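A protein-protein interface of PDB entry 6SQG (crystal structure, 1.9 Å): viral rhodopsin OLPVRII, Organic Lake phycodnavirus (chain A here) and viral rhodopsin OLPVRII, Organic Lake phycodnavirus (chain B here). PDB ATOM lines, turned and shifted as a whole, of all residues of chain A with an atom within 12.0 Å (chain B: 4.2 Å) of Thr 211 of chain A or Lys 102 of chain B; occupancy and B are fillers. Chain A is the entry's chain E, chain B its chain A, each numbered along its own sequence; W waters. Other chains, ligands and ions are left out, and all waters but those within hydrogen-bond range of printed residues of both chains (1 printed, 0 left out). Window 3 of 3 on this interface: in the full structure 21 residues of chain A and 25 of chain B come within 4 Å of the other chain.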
ATOM      1  N   ALA A 156     -14.449  18.388   1.543  1.00  0.00           N
ATOM      2  CA  ALA A 156     -15.201  19.042   2.608  1.00  0.00           C
ATOM      3  C   ALA A 156     -15.714  20.431   2.218  1.00  0.00           C
ATOM      4  O   ALA A 156     -16.846  20.790   2.542  1.00  0.00           O
ATOM      5  CB  ALA A 156     -14.357  19.119   3.876  1.00  0.00           C
ATOM      6  N   LEU A 160     -19.722  21.427   1.448  1.00  0.00           N
ATOM      7  CA  LEU A 160     -20.321  22.490   2.240  1.00  0.00           C
ATOM      8  C   LEU A 160     -20.838  23.585   1.311  1.00  0.00           C
ATOM      9  O   LEU A 160     -21.949  24.078   1.481  1.00  0.00           O
ATOM     10  CB  LEU A 160     -19.306  23.080   3.223  1.00  0.00           C
ATOM     11  CG  LEU A 160     -19.758  24.356   3.950  1.00  0.00           C
ATOM     12  CD1 LEU A 160     -20.942  24.091   4.873  1.00  0.00           C
ATOM     13  CD2 LEU A 160     -18.614  24.962   4.749  1.00  0.00           C
ATOM     14  N   TYR A 201     -16.858  33.379   4.143  1.00  0.00           N
ATOM     15  CA  TYR A 201     -16.355  32.016   4.139  1.00  0.00           C
ATOM     16  C   TYR A 201     -15.195  31.846   3.158  1.00  0.00           C
ATOM     17  O   TYR A 201     -14.164  31.266   3.502  1.00  0.00           O
ATOM     18  CB  TYR A 201     -17.466  30.999   3.805  1.00  0.00           C
ATOM     19  CG  TYR A 201     -16.895  29.627   3.490  1.00  0.00           C
ATOM     20  CD1 TYR A 201     -16.594  28.722   4.503  1.00  0.00           C
ATOM     21  CD2 TYR A 201     -16.606  29.264   2.187  1.00  0.00           C
ATOM     22  CE1 TYR A 201     -16.049  27.480   4.218  1.00  0.00           C
ATOM     23  CE2 TYR A 201     -16.069  28.026   1.892  1.00  0.00           C
ATOM     24  CZ  TYR A 201     -15.791  27.141   2.911  1.00  0.00           C
ATOM     25  OH  TYR A 201     -15.246  25.918   2.603  1.00  0.00           O
ATOM     26  N   TRP A 203     -13.111  34.082   1.984  1.00  0.00           N
ATOM     27  CA  TRP A 203     -11.951  34.780   2.520  1.00  0.00           C
ATOM     28  C   TRP A 203     -11.291  33.973   3.647  1.00  0.00           C
ATOM     29  O   TRP A 203     -10.087  33.692   3.618  1.00  0.00           O
ATOM     30  CB  TRP A 203     -12.361  36.150   3.044  1.00  0.00           C
ATOM     31  CG  TRP A 203     -11.264  36.784   3.812  1.00  0.00           C
ATOM     32  CD1 TRP A 203     -10.173  37.416   3.299  1.00  0.00           C
ATOM     33  CD2 TRP A 203     -11.132  36.837   5.232  1.00  0.00           C
ATOM     34  NE1 TRP A 203      -9.364  37.856   4.313  1.00  0.00           N
ATOM     35  CE2 TRP A 203      -9.932  37.515   5.512  1.00  0.00           C
ATOM     36  CE3 TRP A 203     -11.903  36.370   6.294  1.00  0.00           C
ATOM     37  CZ2 TRP A 203      -9.488  37.738   6.808  1.00  0.00           C
ATOM     38  CZ3 TRP A 203     -11.451  36.583   7.588  1.00  0.00           C
ATOM     39  CH2 TRP A 203     -10.264  37.268   7.830  1.00  0.00           C
ATOM     40  N   ALA A 204     -12.098  33.586   4.628  1.00  0.00           N
ATOM     41  CA  ALA A 204     -11.612  32.854   5.780  1.00  0.00           C
ATOM     42  C   ALA A 204     -10.997  31.514   5.377  1.00  0.00           C
ATOM     43  O   ALA A 204      -9.987  31.101   5.945  1.00  0.00           O
ATOM     44  CB  ALA A 204     -12.733  32.657   6.782  1.00  0.00           C
ATOM     45  N   PHE A 205     -11.595  30.855   4.385  1.00  0.00           N
ATOM     46  CA  PHE A 205     -11.119  29.560   3.926  1.00  0.00           C
ATOM     47  C   PHE A 205      -9.743  29.688   3.291  1.00  0.00           C
ATOM     48  O   PHE A 205      -8.813  28.965   3.664  1.00  0.00           O
ATOM     49  CB  PHE A 205     -12.114  28.940   2.931  1.00  0.00           C
ATOM     50  CG  PHE A 205     -11.684  27.600   2.399  1.00  0.00           C
ATOM     51  CD1 PHE A 205     -11.682  26.482   3.220  1.00  0.00           C
ATOM     52  CD2 PHE A 205     -11.271  27.461   1.086  1.00  0.00           C
ATOM     53  CE1 PHE A 205     -11.275  25.246   2.740  1.00  0.00           C
ATOM     54  CE2 PHE A 205     -10.872  26.225   0.594  1.00  0.00           C
ATOM     55  CZ  PHE A 205     -10.874  25.117   1.425  1.00  0.00           C
ATOM     56  N   TYR A 206      -9.598  30.614   2.343  1.00  0.00           N
ATOM     57  CA  TYR A 206      -8.317  30.791   1.662  1.00  0.00           C
ATOM     58  C   TYR A 206      -7.244  31.405   2.560  1.00  0.00           C
ATOM     59  O   TYR A 206      -6.060  31.137   2.382  1.00  0.00           O
ATOM     60  CB  TYR A 206      -8.484  31.620   0.393  1.00  0.00           C
ATOM     61  CG  TYR A 206      -9.376  30.946  -0.621  1.00  0.00           C
ATOM     62  CD1 TYR A 206      -9.157  29.624  -0.997  1.00  0.00           C
ATOM     63  CD2 TYR A 206     -10.441  31.625  -1.196  1.00  0.00           C
ATOM     64  CE1 TYR A 206      -9.977  28.995  -1.913  1.00  0.00           C
ATOM     65  CE2 TYR A 206     -11.264  31.007  -2.112  1.00  0.00           C
ATOM     66  CZ  TYR A 206     -11.032  29.696  -2.464  1.00  0.00           C
ATOM     67  OH  TYR A 206     -11.859  29.102  -3.383  1.00  0.00           O
ATOM     68  N   ALA A 207      -7.667  32.217   3.521  1.00  0.00           N
ATOM     69  CA  ALA A 207      -6.738  32.820   4.485  1.00  0.00           C
ATOM     70  C   ALA A 207      -6.337  31.870   5.616  1.00  0.00           C
ATOM     71  O   ALA A 207      -5.438  32.194   6.392  1.00  0.00           O
ATOM     72  CB  ALA A 207      -7.346  34.079   5.068  1.00  0.00           C
ATOM     73  N   LYS A 208      -7.023  30.730   5.729  1.00  0.00           N
ATOM     74  CA  LYS A 208      -6.730  29.712   6.751  1.00  0.00           C
ATOM     75  C   LYS A 208      -6.869  30.241   8.182  1.00  0.00           C
ATOM     76  O   LYS A 208      -6.070  29.938   9.071  1.00  0.00           O
ATOM     77  CB  LYS A 208      -5.339  29.113   6.516  1.00  0.00           C
ATOM     78  CG  LYS A 208      -5.176  28.563   5.108  1.00  0.00           C
ATOM     79  CD  LYS A 208      -4.024  27.578   4.985  1.00  0.00           C
ATOM     80  CE  LYS A 208      -2.685  28.290   4.952  1.00  0.00           C
ATOM     81  N   ILE A 209      -7.927  31.010   8.391  1.00  0.00           N
ATOM     82  CA  ILE A 209      -8.213  31.687   9.654  1.00  0.00           C
ATOM     83  C   ILE A 209      -8.695  30.701  10.718  1.00  0.00           C
ATOM     84  O   ILE A 209      -8.454  30.876  11.914  1.00  0.00           O
ATOM     85  CB  ILE A 209      -9.321  32.749   9.411  1.00  0.00           C
ATOM     86  CG1 ILE A 209      -8.803  33.857   8.488  1.00  0.00           C
ATOM     87  CG2 ILE A 209      -9.840  33.333  10.711  1.00  0.00           C
ATOM     88  CD1 ILE A 209      -7.594  34.590   9.026  1.00  0.00           C
ATOM     89  N   PHE A 210      -9.389  29.659  10.287  1.00  0.00           N
ATOM     90  CA  PHE A 210     -10.038  28.765  11.228  1.00  0.00           C
ATOM     91  C   PHE A 210      -9.455  27.361  11.203  1.00  0.00           C
ATOM     92  O   PHE A 210      -9.159  26.828  10.143  1.00  0.00           O
ATOM     93  CB  PHE A 210     -11.540  28.711  10.937  1.00  0.00           C
ATOM     94  CG  PHE A 210     -12.262  29.994  11.250  1.00  0.00           C
ATOM     95  CD1 PHE A 210     -12.342  30.452  12.548  1.00  0.00           C
ATOM     96  CD2 PHE A 210     -12.854  30.741  10.244  1.00  0.00           C
ATOM     97  CE1 PHE A 210     -13.002  31.633  12.846  1.00  0.00           C
ATOM     98  CE2 PHE A 210     -13.512  31.920  10.534  1.00  0.00           C
ATOM     99  CZ  PHE A 210     -13.589  32.366  11.836  1.00  0.00           C
ATOM    100  N   THR A 211      -9.297  26.768  12.383  1.00  0.00           N
ATOM    101  CA  THR A 211      -9.004  25.335  12.490  1.00  0.00           C
ATOM    102  C   THR A 211     -10.333  24.606  12.741  1.00  0.00           C
ATOM    103  O   THR A 211     -11.125  25.019  13.592  1.00  0.00           O
ATOM    104  CB  THR A 211      -8.036  25.036  13.649  1.00  0.00           C
ATOM    105  OG1 THR A 211      -7.124  26.126  13.816  1.00  0.00           O
ATOM    106  CG2 THR A 211      -7.257  23.764  13.382  1.00  0.00           C
ATOM    107  N   LEU A 212     -10.584  23.536  11.995  1.00  0.00           N
ATOM    108  CA  LEU A 212     -11.822  22.771  12.158  1.00  0.00           C
ATOM    109  C   LEU A 212     -11.677  21.752  13.281  1.00  0.00           C
ATOM    110  O   LEU A 212     -10.847  20.848  13.200  1.00  0.00           O
ATOM    111  CB  LEU A 212     -12.193  22.075  10.859  1.00  0.00           C
ATOM    112  N   MET B 100      -4.801  32.300  13.544  1.00  0.00           N
ATOM    113  CA  MET B 100      -5.746  31.197  13.516  1.00  0.00           C
ATOM    114  C   MET B 100      -6.472  31.094  14.837  1.00  0.00           C
ATOM    115  O   MET B 100      -5.939  31.442  15.896  1.00  0.00           O
ATOM    116  CB  MET B 100      -5.041  29.863  13.276  1.00  0.00           C
ATOM    117  CG  MET B 100      -4.474  29.665  11.890  1.00  0.00           C
ATOM    118  SD  MET B 100      -4.179  27.915  11.577  1.00  0.00           S
ATOM    119  CE  MET B 100      -3.659  27.977   9.861  1.00  0.00           C
ATOM    120  N   VAL B 101      -7.689  30.581  14.765  1.00  0.00           N
ATOM    121  CA  VAL B 101      -8.450  30.253  15.953  1.00  0.00           C
ATOM    122  C   VAL B 101      -9.322  29.049  15.604  1.00  0.00           C
ATOM    123  O   VAL B 101      -9.636  28.836  14.427  1.00  0.00           O
ATOM    124  CB  VAL B 101      -9.311  31.450  16.402  1.00  0.00           C
ATOM    125  CG1 VAL B 101     -10.397  31.764  15.374  1.00  0.00           C
ATOM    126  CG2 VAL B 101      -9.912  31.185  17.776  1.00  0.00           C
ATOM    127  N   LYS B 102      -9.707  28.252  16.602  1.00  0.00           N
ATOM    128  CA  LYS B 102     -10.673  27.176  16.363  1.00  0.00           C
ATOM    129  C   LYS B 102     -12.047  27.775  16.102  1.00  0.00           C
ATOM    130  O   LYS B 102     -12.508  28.631  16.855  1.00  0.00           O
ATOM    131  CB  LYS B 102     -10.769  26.231  17.558  1.00  0.00           C
ATOM    132  CG  LYS B 102      -9.573  25.324  17.756  1.00  0.00           C
ATOM    133  CD  LYS B 102      -9.912  24.215  18.747  1.00  0.00           C
ATOM    134  CE  LYS B 102      -8.665  23.495  19.241  1.00  0.00           C
ATOM    135  N   PHE B 103     -12.699  27.322  15.041  1.00  0.00           N
ATOM    136  CA  PHE B 103     -14.026  27.817  14.697  1.00  0.00           C
ATOM    137  C   PHE B 103     -15.027  27.596  15.830  1.00  0.00           C
ATOM    138  O   PHE B 103     -15.859  28.461  16.098  1.00  0.00           O
ATOM    139  CB  PHE B 103     -14.544  27.162  13.410  1.00  0.00           C
ATOM    140  CG  PHE B 103     -15.814  27.783  12.887  1.00  0.00           C
ATOM    141  CD1 PHE B 103     -15.816  29.084  12.409  1.00  0.00           C
ATOM    142  CD2 PHE B 103     -17.003  27.070  12.881  1.00  0.00           C
ATOM    143  CE1 PHE B 103     -16.980  29.667  11.937  1.00  0.00           C
ATOM    144  CE2 PHE B 103     -18.167  27.642  12.403  1.00  0.00           C
ATOM    145  CZ  PHE B 103     -18.156  28.945  11.933  1.00  0.00           C
ATOM    146  N   SER B 104     -14.944  26.444  16.493  1.00  0.00           N
ATOM    147  CA  SER B 104     -15.841  26.148  17.610  1.00  0.00           C
ATOM    148  C   SER B 104     -15.667  27.164  18.746  1.00  0.00           C
ATOM    149  O   SER B 104     -16.646  27.633  19.326  1.00  0.00           O
ATOM    150  CB  SER B 104     -15.628  24.711  18.122  1.00  0.00           C
ATOM    151  OG  SER B 104     -14.266  24.457  18.427  1.00  0.00           O
ATOM    152  N   ASP B 105     -14.425  27.507  19.065  1.00  0.00           N
ATOM    153  CA  ASP B 105     -14.164  28.530  20.072  1.00  0.00           C
ATOM    154  C   ASP B 105     -14.778  29.858  19.645  1.00  0.00           C
ATOM    155  O   ASP B 105     -15.393  30.557  20.446  1.00  0.00           O
ATOM    156  CB  ASP B 105     -12.667  28.718  20.276  1.00  0.00           C
ATOM    157  CG  ASP B 105     -12.051  27.628  21.121  1.00  0.00           C
ATOM    158  OD1 ASP B 105     -12.803  26.873  21.769  1.00  0.00           O
ATOM    159  OD2 ASP B 105     -10.811  27.545  21.147  1.00  0.00           O
ATOM    160  N   PHE B 106     -14.608  30.208  18.377  1.00  0.00           N
ATOM    161  CA  PHE B 106     -15.146  31.452  17.887  1.00  0.00           C
ATOM    162  C   PHE B 106     -16.678  31.455  17.947  1.00  0.00           C
ATOM    163  O   PHE B 106     -17.294  32.462  18.296  1.00  0.00           O
ATOM    164  CB  PHE B 106     -14.633  31.750  16.476  1.00  0.00           C
ATOM    165  CG  PHE B 106     -15.093  33.074  15.942  1.00  0.00           C
ATOM    166  CD1 PHE B 106     -14.829  34.243  16.640  1.00  0.00           C
ATOM    167  CD2 PHE B 106     -15.793  33.152  14.751  1.00  0.00           C
ATOM    168  CE1 PHE B 106     -15.265  35.467  16.161  1.00  0.00           C
ATOM    169  CE2 PHE B 106     -16.229  34.376  14.265  1.00  0.00           C
ATOM    170  CZ  PHE B 106     -15.965  35.534  14.974  1.00  0.00           C
HETATM  171  O   HOH W   1     -13.433  24.062  15.448  1.00  0.00           O
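The backbone carbonyl oxygen (O) of Val 101 of chain B sits at hydrogen-bond distance from the backbone NH (N) of Thr 211 of chain A (2.9 Å). O of Lys 208 of chain A lies close to SD of Met 100 of chain B (3.7 Å). N of Val 101 of chain B lies within hydrogen-bond range of O of Ile 209 of chain A (3.0 Å). The backbone NH (N) of Phe 103 of chain B sits at hydrogen-bond distance from the backbone carbonyl oxygen (O) of Thr 211 of chain A (3.1 Å).
Water W1 lies within hydrogen-bond range of N of Ser 104 of chain B, O of Thr 211 of chain A and N of Phe 103 of chain B.
Of the 13 printed residues of chain A, 4 touch a printed residue of chain B. Printed residues of chain A that touch a printed residue of chain B: Lys 208, Ile 209, Phe 210 and Thr 211. Hydrophobic or aromatic side chains of chain A that line the printed part of chain B: Phe 210. Of the 7 printed residues of chain B, 5 touch a printed residue of chain A. Hydrophobic or aromatic side chains of chain B that line the printed part of chain A: Met 100, Val 101, Phe 103 and Phe 106.
Ile 209 of chain A touches Met 100 of chain B (O to CA, 3.2 Å). Val 101 of chain B touches Phe 210 of chain A (O to CA, 3.2 Å). Phe 103 of chain B touches Phe 210 of chain A (CD1 to CD1, 3.7 Å). CD2 of Phe 106 of chain B touches CE1 of Phe 210 of chain A, 3.7 Å away. O of Thr 211 of chain A touches CA of Lys 102 of chain B, 3.5 Å away.
The backbone carbonyl oxygen (O) of Ala 204 of chain A lies within hydrogen-bond range of the backbone NH (N) of Ile 209 of chain A (3.2 Å).
Of the printed residues of chain B, Lys 208 of chain A touches Met 100 (3.2 Å). Of the printed residues of chain B, Ile 209 of chain A touches Met 100 (3.2 Å) and Val 101 (3.0 Å). Printed residues of chain B within 4 Å of Phe 210 of chain A: Val 101, Phe 103 and Phe 106. Thr 211 of chain A touches three residues of chain B. Met 100 of chain B touches just these residues of chain A: Lys 208 and Ile 209. Val 101 of chain B touches just these residues of chain A: Ile 209, Phe 210 and Thr 211. Printed residues of chain A within 4 Å of Lys 102 of chain B: Thr 211. Printed residues of chain A within 4 Å of Phe 103 of chain B: Phe 210 (3.7 Å) and Thr 211 (3.1 Å). Ser 104 of chain B touches none of the printed residues of chain A. No residue of chain A comes within 4 Å of Asp 105 of chain B. Phe 106 of chain B touches just one residue of chain A: Phe 210. The nearest residue of chain A that does not touch Lys 102 of chain B is Phe 210 of chain A (4.5 Å).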
